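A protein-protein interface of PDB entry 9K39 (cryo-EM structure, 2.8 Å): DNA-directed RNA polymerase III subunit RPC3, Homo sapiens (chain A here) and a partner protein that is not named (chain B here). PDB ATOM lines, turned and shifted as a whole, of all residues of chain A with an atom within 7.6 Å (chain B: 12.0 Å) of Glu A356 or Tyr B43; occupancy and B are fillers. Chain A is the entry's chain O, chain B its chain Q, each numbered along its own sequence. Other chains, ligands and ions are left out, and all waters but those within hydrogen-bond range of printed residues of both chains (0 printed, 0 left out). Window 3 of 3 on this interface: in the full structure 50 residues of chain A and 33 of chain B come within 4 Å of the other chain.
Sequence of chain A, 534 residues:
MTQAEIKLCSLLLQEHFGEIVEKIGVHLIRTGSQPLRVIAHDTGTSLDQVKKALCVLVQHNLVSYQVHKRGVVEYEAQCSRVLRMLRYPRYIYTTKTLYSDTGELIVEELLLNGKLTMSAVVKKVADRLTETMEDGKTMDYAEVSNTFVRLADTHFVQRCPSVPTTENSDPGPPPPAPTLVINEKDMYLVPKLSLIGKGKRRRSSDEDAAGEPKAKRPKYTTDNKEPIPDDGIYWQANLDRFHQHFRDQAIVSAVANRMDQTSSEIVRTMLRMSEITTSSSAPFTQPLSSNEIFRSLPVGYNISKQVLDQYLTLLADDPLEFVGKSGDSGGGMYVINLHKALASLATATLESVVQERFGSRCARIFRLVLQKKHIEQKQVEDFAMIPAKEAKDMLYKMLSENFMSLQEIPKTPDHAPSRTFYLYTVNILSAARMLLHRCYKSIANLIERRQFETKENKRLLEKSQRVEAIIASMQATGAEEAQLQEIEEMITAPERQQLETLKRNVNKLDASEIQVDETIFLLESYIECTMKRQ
The backbone carbonyl oxygen (O) of Phe A358 is in hydrogen-bond range of the side-chain hydroxyl (OH) of Tyr B43 (3.2 Å).
OG1 of Thr B41 is in hydrogen-bond range of O of Tyr B43 (3.4 Å).
Among the printed residues, merely in contact across the chains: Glu A356 with Tyr B43, Glu A356 with Val B46, Arg A357 with Tyr B43 and Gly A359 with Tyr B43.
Of chain B, only Tyr B43 (3.9 Å) and Val B46 (2.9 Å) come within 4 Å of Glu A356.
Tyr B43 touches just these residues of chain A: Glu A356, Arg A357, Phe A358 and Gly A359.
Ser A352 touches none of the printed residues of chain B.
No residue of chain B comes within 4 Å of Val A354.
Gln A355 touches none of the printed residues of chain B.
No residue of chain B comes within 4 Å of Ser A360.
Printed residues of chain A within 4 Å of Val B46: Glu A356.
Printed residues of chain B within 4 Å of Arg A357: Tyr B43 (3.8 Å).
Leu A350 touches none of the printed residues of chain B.
Pro B39 touches none of the printed residues of chain A.
The nearest residue of chain A that does not touch Tyr B43 is Ser A360 (4.7 Å).
The nearest printed residue of chain A that does not touch Val B46 is Ser A352 (7.0 Å).
Of the 17 printed residues of chain A, 4 touch a printed residue of chain B.
Of the 12 printed residues of chain B, 2 touch a printed residue of chain A.
Among the printed residues, no Asp or Glu carboxylate lies within 4 Å of a Lys or Arg side-chain nitrogen of the other chain.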
ATOM      1  N   LEU A 350      14.996 -18.738   0.128  1.00  0.00           N
ATOM      2  CA  LEU A 350      16.112 -18.960   1.043  1.00  0.00           C
ATOM      3  C   LEU A 350      16.222 -20.430   1.436  1.00  0.00           C
ATOM      4  O   LEU A 350      17.323 -20.994   1.453  1.00  0.00           O
ATOM      5  CB  LEU A 350      15.957 -18.076   2.281  1.00  0.00           C
ATOM      6  CG  LEU A 350      17.171 -17.966   3.200  1.00  0.00           C
ATOM      7  CD1 LEU A 350      18.409 -17.575   2.411  1.00  0.00           C
ATOM      8  CD2 LEU A 350      16.902 -16.955   4.305  1.00  0.00           C
ATOM      9  N   GLU A 351      15.094 -21.074   1.742  1.00  0.00           N
ATOM     10  CA  GLU A 351      15.152 -22.485   2.102  1.00  0.00           C
ATOM     11  C   GLU A 351      15.574 -23.336   0.910  1.00  0.00           C
ATOM     12  O   GLU A 351      16.290 -24.328   1.074  1.00  0.00           O
ATOM     13  CB  GLU A 351      13.808 -22.953   2.669  1.00  0.00           C
ATOM     14  CG  GLU A 351      12.668 -23.013   1.668  1.00  0.00           C
ATOM     15  CD  GLU A 351      11.368 -23.478   2.293  1.00  0.00           C
ATOM     16  OE1 GLU A 351      11.319 -23.619   3.533  1.00  0.00           O
ATOM     17  OE2 GLU A 351      10.393 -23.700   1.544  1.00  0.00           O
ATOM     18  N   SER A 352      15.180 -22.939  -0.304  1.00  0.00           N
ATOM     19  CA  SER A 352      15.583 -23.685  -1.490  1.00  0.00           C
ATOM     20  C   SER A 352      17.080 -23.563  -1.741  1.00  0.00           C
ATOM     21  O   SER A 352      17.744 -24.557  -2.061  1.00  0.00           O
ATOM     22  CB  SER A 352      14.792 -23.202  -2.706  1.00  0.00           C
ATOM     23  OG  SER A 352      15.176 -23.904  -3.875  1.00  0.00           O
ATOM     24  N   VAL A 353      17.636 -22.356  -1.600  1.00  0.00           N
ATOM     25  CA  VAL A 353      19.070 -22.197  -1.828  1.00  0.00           C
ATOM     26  C   VAL A 353      19.864 -22.898  -0.727  1.00  0.00           C
ATOM     27  O   VAL A 353      20.918 -23.487  -0.991  1.00  0.00           O
ATOM     28  CB  VAL A 353      19.448 -20.708  -1.965  1.00  0.00           C
ATOM     29  CG1 VAL A 353      19.224 -19.948  -0.674  1.00  0.00           C
ATOM     30  CG2 VAL A 353      20.897 -20.568  -2.418  1.00  0.00           C
ATOM     31  N   VAL A 354      19.352 -22.894   0.507  1.00  0.00           N
ATOM     32  CA  VAL A 354      20.013 -23.633   1.580  1.00  0.00           C
ATOM     33  C   VAL A 354      19.999 -25.130   1.285  1.00  0.00           C
ATOM     34  O   VAL A 354      21.010 -25.821   1.456  1.00  0.00           O
ATOM     35  CB  VAL A 354      19.356 -23.313   2.938  1.00  0.00           C
ATOM     36  CG1 VAL A 354      19.801 -24.313   3.996  1.00  0.00           C
ATOM     37  CG2 VAL A 354      19.702 -21.897   3.368  1.00  0.00           C
ATOM     38  N   GLN A 355      18.854 -25.651   0.830  1.00  0.00           N
ATOM     39  CA  GLN A 355      18.756 -27.070   0.512  1.00  0.00           C
ATOM     40  C   GLN A 355      19.694 -27.452  -0.624  1.00  0.00           C
ATOM     41  O   GLN A 355      20.350 -28.501  -0.574  1.00  0.00           O
ATOM     42  CB  GLN A 355      17.314 -27.428   0.153  1.00  0.00           C
ATOM     43  CG  GLN A 355      17.091 -28.902  -0.139  1.00  0.00           C
ATOM     44  CD  GLN A 355      15.641 -29.224  -0.447  1.00  0.00           C
ATOM     45  OE1 GLN A 355      14.770 -28.359  -0.362  1.00  0.00           O
ATOM     46  NE2 GLN A 355      15.378 -30.475  -0.807  1.00  0.00           N
ATOM     47  N   GLU A 356      19.773 -26.617  -1.661  1.00  0.00           N
ATOM     48  CA  GLU A 356      20.619 -26.939  -2.802  1.00  0.00           C
ATOM     49  C   GLU A 356      22.099 -26.703  -2.525  1.00  0.00           C
ATOM     50  O   GLU A 356      22.942 -27.246  -3.247  1.00  0.00           O
ATOM     51  CB  GLU A 356      20.180 -26.136  -4.027  1.00  0.00           C
ATOM     52  CG  GLU A 356      18.813 -26.522  -4.566  1.00  0.00           C
ATOM     53  CD  GLU A 356      18.788 -27.918  -5.163  1.00  0.00           C
ATOM     54  OE1 GLU A 356      19.864 -28.430  -5.538  1.00  0.00           O
ATOM     55  OE2 GLU A 356      17.689 -28.506  -5.257  1.00  0.00           O
ATOM     56  N   ARG A 357      22.437 -25.909  -1.507  1.00  0.00           N
ATOM     57  CA  ARG A 357      23.840 -25.664  -1.205  1.00  0.00           C
ATOM     58  C   ARG A 357      24.397 -26.597  -0.137  1.00  0.00           C
ATOM     59  O   ARG A 357      25.589 -26.921  -0.175  1.00  0.00           O
ATOM     60  CB  ARG A 357      24.037 -24.209  -0.765  1.00  0.00           C
ATOM     61  CG  ARG A 357      25.495 -23.793  -0.631  1.00  0.00           C
ATOM     62  CD  ARG A 357      25.628 -22.324  -0.270  1.00  0.00           C
ATOM     63  NE  ARG A 357      27.023 -21.937  -0.081  1.00  0.00           N
ATOM     64  CZ  ARG A 357      27.417 -20.723   0.294  1.00  0.00           C
ATOM     65  NH1 ARG A 357      26.516 -19.776   0.520  1.00  0.00           N
ATOM     66  NH2 ARG A 357      28.707 -20.457   0.441  1.00  0.00           N
ATOM     67  N   PHE A 358      23.567 -27.055   0.805  1.00  0.00           N
ATOM     68  CA  PHE A 358      24.062 -27.876   1.903  1.00  0.00           C
ATOM     69  C   PHE A 358      23.282 -29.164   2.128  1.00  0.00           C
ATOM     70  O   PHE A 358      23.572 -29.875   3.096  1.00  0.00           O
ATOM     71  CB  PHE A 358      24.077 -27.070   3.211  1.00  0.00           C
ATOM     72  CG  PHE A 358      24.925 -25.833   3.153  1.00  0.00           C
ATOM     73  CD1 PHE A 358      26.304 -25.921   3.203  1.00  0.00           C
ATOM     74  CD2 PHE A 358      24.338 -24.580   3.062  1.00  0.00           C
ATOM     75  CE1 PHE A 358      27.087 -24.782   3.155  1.00  0.00           C
ATOM     76  CE2 PHE A 358      25.113 -23.441   3.016  1.00  0.00           C
ATOM     77  CZ  PHE A 358      26.491 -23.541   3.062  1.00  0.00           C
ATOM     78  N   GLY A 359      22.311 -29.485   1.281  1.00  0.00           N
ATOM     79  CA  GLY A 359      21.577 -30.728   1.396  1.00  0.00           C
ATOM     80  C   GLY A 359      20.225 -30.552   2.064  1.00  0.00           C
ATOM     81  O   GLY A 359      19.831 -29.463   2.488  1.00  0.00           O
ATOM     82  N   SER A 360      19.502 -31.671   2.155  1.00  0.00           N
ATOM     83  CA  SER A 360      18.152 -31.646   2.709  1.00  0.00           C
ATOM     84  C   SER A 360      18.158 -31.580   4.232  1.00  0.00           C
ATOM     85  O   SER A 360      17.246 -30.994   4.826  1.00  0.00           O
ATOM     86  CB  SER A 360      17.365 -32.869   2.236  1.00  0.00           C
ATOM     87  OG  SER A 360      17.263 -32.893   0.823  1.00  0.00           O
ATOM     88  N   ARG A 361      19.164 -32.175   4.881  1.00  0.00           N
ATOM     89  CA  ARG A 361      19.218 -32.138   6.339  1.00  0.00           C
ATOM     90  C   ARG A 361      19.503 -30.730   6.845  1.00  0.00           C
ATOM     91  O   ARG A 361      18.915 -30.286   7.842  1.00  0.00           O
ATOM     92  CB  ARG A 361      20.276 -33.118   6.846  1.00  0.00           C
ATOM     93  CG  ARG A 361      20.118 -34.528   6.298  1.00  0.00           C
ATOM     94  CD  ARG A 361      21.219 -35.450   6.796  1.00  0.00           C
ATOM     95  NE  ARG A 361      21.132 -35.681   8.234  1.00  0.00           N
ATOM     96  CZ  ARG A 361      20.450 -36.677   8.793  1.00  0.00           C
ATOM     97  NH1 ARG A 361      19.790 -37.538   8.032  1.00  0.00           N
ATOM     98  NH2 ARG A 361      20.427 -36.810  10.113  1.00  0.00           N
ATOM     99  N   CYS A 362      20.403 -30.008   6.171  1.00  0.00           N
ATOM    100  CA  CYS A 362      20.651 -28.621   6.540  1.00  0.00           C
ATOM    101  C   CYS A 362      19.420 -27.763   6.298  1.00  0.00           C
ATOM    102  O   CYS A 362      19.144 -26.830   7.061  1.00  0.00           O
ATOM    103  CB  CYS A 362      21.851 -28.077   5.766  1.00  0.00           C
ATOM    104  SG  CYS A 362      22.341 -26.405   6.242  1.00  0.00           S
ATOM    105  N   ALA A 363      18.655 -28.068   5.247  1.00  0.00           N
ATOM    106  CA  ALA A 363      17.400 -27.360   5.020  1.00  0.00           C
ATOM    107  C   ALA A 363      16.394 -27.658   6.123  1.00  0.00           C
ATOM    108  O   ALA A 363      15.628 -26.777   6.532  1.00  0.00           O
ATOM    109  CB  ALA A 363      16.825 -27.732   3.656  1.00  0.00           C
ATOM    110  N   GLU A 390      27.069 -33.775  13.582  1.00  0.00           N
ATOM    111  CA  GLU A 390      26.667 -33.423  12.225  1.00  0.00           C
ATOM    112  C   GLU A 390      25.750 -32.213  12.172  1.00  0.00           C
ATOM    113  O   GLU A 390      25.924 -31.355  11.305  1.00  0.00           O
ATOM    114  CB  GLU A 390      25.974 -34.618  11.552  1.00  0.00           C
ATOM    115  CG  GLU A 390      25.539 -34.356  10.119  1.00  0.00           C
ATOM    116  CD  GLU A 390      24.873 -35.559   9.480  1.00  0.00           C
ATOM    117  OE1 GLU A 390      24.798 -36.618  10.140  1.00  0.00           O
ATOM    118  OE2 GLU A 390      24.423 -35.447   8.320  1.00  0.00           O
ATOM    119  N   MET A 394      26.630 -28.440  10.510  1.00  0.00           N
ATOM    120  CA  MET A 394      25.832 -27.665   9.564  1.00  0.00           C
ATOM    121  C   MET A 394      25.452 -26.308  10.146  1.00  0.00           C
ATOM    122  O   MET A 394      25.393 -25.308   9.420  1.00  0.00           O
ATOM    123  CB  MET A 394      24.585 -28.450   9.160  1.00  0.00           C
ATOM    124  CG  MET A 394      24.883 -29.757   8.443  1.00  0.00           C
ATOM    125  SD  MET A 394      23.391 -30.656   7.970  1.00  0.00           S
ATOM    126  CE  MET A 394      24.101 -32.082   7.148  1.00  0.00           C
ATOM    127  N   LYS A 397      28.480 -24.200   9.726  1.00  0.00           N
ATOM    128  CA  LYS A 397      28.632 -23.854   8.317  1.00  0.00           C
ATOM    129  C   LYS A 397      27.682 -22.731   7.918  1.00  0.00           C
ATOM    130  O   LYS A 397      28.073 -21.802   7.201  1.00  0.00           O
ATOM    131  CB  LYS A 397      28.404 -25.089   7.444  1.00  0.00           C
ATOM    132  CG  LYS A 397      29.516 -26.125   7.537  1.00  0.00           C
ATOM    133  CD  LYS A 397      29.188 -27.365   6.724  1.00  0.00           C
ATOM    134  CE  LYS A 397      29.041 -27.039   5.248  1.00  0.00           C
ATOM    135  NZ  LYS A 397      28.715 -28.248   4.442  1.00  0.00           N
ATOM    136  N   PHE B  38      40.607 -25.117  -5.166  1.00  0.00           N
ATOM    137  CA  PHE B  38      39.178 -25.302  -5.419  1.00  0.00           C
ATOM    138  C   PHE B  38      38.744 -26.612  -4.777  1.00  0.00           C
ATOM    139  O   PHE B  38      38.828 -27.680  -5.404  1.00  0.00           O
ATOM    140  CB  PHE B  38      38.880 -25.293  -6.918  1.00  0.00           C
ATOM    141  CG  PHE B  38      39.220 -23.996  -7.596  1.00  0.00           C
ATOM    142  CD1 PHE B  38      40.483 -23.784  -8.126  1.00  0.00           C
ATOM    143  CD2 PHE B  38      38.277 -22.989  -7.705  1.00  0.00           C
ATOM    144  CE1 PHE B  38      40.797 -22.591  -8.751  1.00  0.00           C
ATOM    145  CE2 PHE B  38      38.584 -21.794  -8.329  1.00  0.00           C
ATOM    146  CZ  PHE B  38      39.848 -21.595  -8.852  1.00  0.00           C
ATOM    147  N   PRO B  39      38.283 -26.582  -3.526  1.00  0.00           N
ATOM    148  CA  PRO B  39      37.861 -27.825  -2.869  1.00  0.00           C
ATOM    149  C   PRO B  39      36.614 -28.405  -3.522  1.00  0.00           C
ATOM    150  O   PRO B  39      35.718 -27.678  -3.953  1.00  0.00           O
ATOM    151  CB  PRO B  39      37.590 -27.387  -1.426  1.00  0.00           C
ATOM    152  CG  PRO B  39      37.276 -25.930  -1.530  1.00  0.00           C
ATOM    153  CD  PRO B  39      38.139 -25.412  -2.644  1.00  0.00           C
ATOM    154  N   ASP B  40      36.566 -29.733  -3.589  1.00  0.00           N
ATOM    155  CA  ASP B  40      35.451 -30.409  -4.232  1.00  0.00           C
ATOM    156  C   ASP B  40      34.203 -30.356  -3.356  1.00  0.00           C
ATOM    157  O   ASP B  40      34.279 -30.326  -2.125  1.00  0.00           O
ATOM    158  CB  ASP B  40      35.814 -31.864  -4.537  1.00  0.00           C
ATOM    159  CG  ASP B  40      36.368 -32.593  -3.329  1.00  0.00           C
ATOM    160  OD1 ASP B  40      36.650 -31.933  -2.307  1.00  0.00           O
ATOM    161  OD2 ASP B  40      36.522 -33.831  -3.400  1.00  0.00           O
ATOM    162  N   THR B  41      33.044 -30.344  -4.008  1.00  0.00           N
ATOM    163  CA  THR B  41      31.756 -30.317  -3.335  1.00  0.00           C
ATOM    164  C   THR B  41      30.885 -31.447  -3.862  1.00  0.00           C
ATOM    165  O   THR B  41      30.849 -31.702  -5.071  1.00  0.00           O
ATOM    166  CB  THR B  41      31.040 -28.973  -3.531  1.00  0.00           C
ATOM    167  OG1 THR B  41      30.879 -28.716  -4.931  1.00  0.00           O
ATOM    168  CG2 THR B  41      31.838 -27.845  -2.899  1.00  0.00           C
ATOM    169  N   ASP B  42      30.182 -32.120  -2.953  1.00  0.00           N
ATOM    170  CA  ASP B  42      29.304 -33.222  -3.323  1.00  0.00           C
ATOM    171  C   ASP B  42      27.961 -32.757  -3.869  1.00  0.00           C
ATOM    172  O   ASP B  42      27.201 -33.586  -4.385  1.00  0.00           O
ATOM    173  CB  ASP B  42      29.082 -34.141  -2.118  1.00  0.00           C
ATOM    174  CG  ASP B  42      28.691 -33.375  -0.871  1.00  0.00           C
ATOM    175  OD1 ASP B  42      28.778 -32.130  -0.886  1.00  0.00           O
ATOM    176  OD2 ASP B  42      28.299 -34.020   0.125  1.00  0.00           O
ATOM    177  N   TYR B  43      27.647 -31.470  -3.774  1.00  0.00           N
ATOM    178  CA  TYR B  43      26.410 -30.914  -4.305  1.00  0.00           C
ATOM    179  C   TYR B  43      26.713 -30.151  -5.588  1.00  0.00           C
ATOM    180  O   TYR B  43      27.607 -29.301  -5.613  1.00  0.00           O
ATOM    181  CB  TYR B  43      25.734 -29.992  -3.287  1.00  0.00           C
ATOM    182  CG  TYR B  43      25.288 -30.697  -2.026  1.00  0.00           C
ATOM    183  CD1 TYR B  43      24.110 -31.433  -1.998  1.00  0.00           C
ATOM    184  CD2 TYR B  43      26.042 -30.621  -0.863  1.00  0.00           C
ATOM    185  CE1 TYR B  43      23.700 -32.078  -0.847  1.00  0.00           C
ATOM    186  CE2 TYR B  43      25.640 -31.263   0.294  1.00  0.00           C
ATOM    187  CZ  TYR B  43      24.466 -31.989   0.298  1.00  0.00           C
ATOM    188  OH  TYR B  43      24.062 -32.629   1.445  1.00  0.00           O
ATOM    189  N   LYS B  44      25.972 -30.460  -6.643  1.00  0.00           N
ATOM    190  CA  LYS B  44      26.152 -29.845  -7.945  1.00  0.00           C
ATOM    191  C   LYS B  44      25.019 -28.871  -8.239  1.00  0.00           C
ATOM    192  O   LYS B  44      23.914 -29.006  -7.702  1.00  0.00           O
ATOM    193  CB  LYS B  44      26.214 -30.914  -9.044  1.00  0.00           C
ATOM    194  CG  LYS B  44      27.265 -31.989  -8.806  1.00  0.00           C
ATOM    195  CD  LYS B  44      28.653 -31.388  -8.645  1.00  0.00           C
ATOM    196  CE  LYS B  44      29.112 -30.698  -9.920  1.00  0.00           C
ATOM    197  NZ  LYS B  44      30.462 -30.088  -9.764  1.00  0.00           N
ATOM    198  N   PRO B  45      25.262 -27.864  -9.078  1.00  0.00           N
ATOM    199  CA  PRO B  45      24.201 -26.905  -9.404  1.00  0.00           C
ATOM    200  C   PRO B  45      23.023 -27.584 -10.087  1.00  0.00           C
ATOM    201  O   PRO B  45      23.190 -28.512 -10.884  1.00  0.00           O
ATOM    202  CB  PRO B  45      24.897 -25.908 -10.337  1.00  0.00           C
ATOM    203  CG  PRO B  45      26.344 -26.016  -9.993  1.00  0.00           C
ATOM    204  CD  PRO B  45      26.561 -27.459  -9.645  1.00  0.00           C
ATOM    205  N   VAL B  46      21.822 -27.112  -9.760  1.00  0.00           N
ATOM    206  CA  VAL B  46      20.606 -27.654 -10.375  1.00  0.00           C
ATOM    207  C   VAL B  46      20.613 -27.326 -11.862  1.00  0.00           C
ATOM    208  O   VAL B  46      20.987 -26.198 -12.243  1.00  0.00           O
ATOM    209  CB  VAL B  46      19.356 -27.082  -9.685  1.00  0.00           C
ATOM    210  CG1 VAL B  46      18.085 -27.603 -10.337  1.00  0.00           C
ATOM    211  CG2 VAL B  46      19.373 -27.415  -8.200  1.00  0.00           C
ATOM    212  N   PRO B  47      20.244 -28.255 -12.745  1.00  0.00           N
ATOM    213  CA  PRO B  47      20.178 -27.925 -14.172  1.00  0.00           C
ATOM    214  C   PRO B  47      19.187 -26.803 -14.442  1.00  0.00           C
ATOM    215  O   PRO B  47      18.178 -26.649 -13.749  1.00  0.00           O
ATOM    216  CB  PRO B  47      19.729 -29.241 -14.825  1.00  0.00           C
ATOM    217  CG  PRO B  47      19.152 -30.055 -13.705  1.00  0.00           C
ATOM    218  CD  PRO B  47      19.938 -29.674 -12.494  1.00  0.00           C
ATOM    219  N   LEU B  48      19.495 -26.007 -15.464  1.00  0.00           N
ATOM    220  CA  LEU B  48      18.682 -24.846 -15.792  1.00  0.00           C
ATOM    221  C   LEU B  48      17.300 -25.264 -16.276  1.00  0.00           C
ATOM    222  O   LEU B  48      17.102 -26.363 -16.800  1.00  0.00           O
ATOM    223  CB  LEU B  48      19.369 -23.993 -16.861  1.00  0.00           C
ATOM    224  CG  LEU B  48      20.571 -23.135 -16.455  1.00  0.00           C
ATOM    225  CD1 LEU B  48      20.264 -22.340 -15.193  1.00  0.00           C
ATOM    226  CD2 LEU B  48      21.838 -23.968 -16.282  1.00  0.00           C
ATOM    227  N   LYS B  49      16.333 -24.369 -16.087  1.00  0.00           N
ATOM    228  CA  LYS B  49      14.976 -24.617 -16.549  1.00  0.00           C
ATOM    229  C   LYS B  49      14.936 -24.676 -18.070  1.00  0.00           C
ATOM    230  O   LYS B  49      15.644 -23.932 -18.757  1.00  0.00           O
ATOM    231  CB  LYS B  49      14.032 -23.529 -16.038  1.00  0.00           C
ATOM    232  CG  LYS B  49      14.026 -23.370 -14.526  1.00  0.00           C
ATOM    233  CD  LYS B  49      13.130 -22.218 -14.092  1.00  0.00           C
ATOM    234  CE  LYS B  49      11.685 -22.452 -14.500  1.00  0.00           C
ATOM    235  NZ  LYS B  49      11.121 -23.677 -13.870  1.00  0.00           N
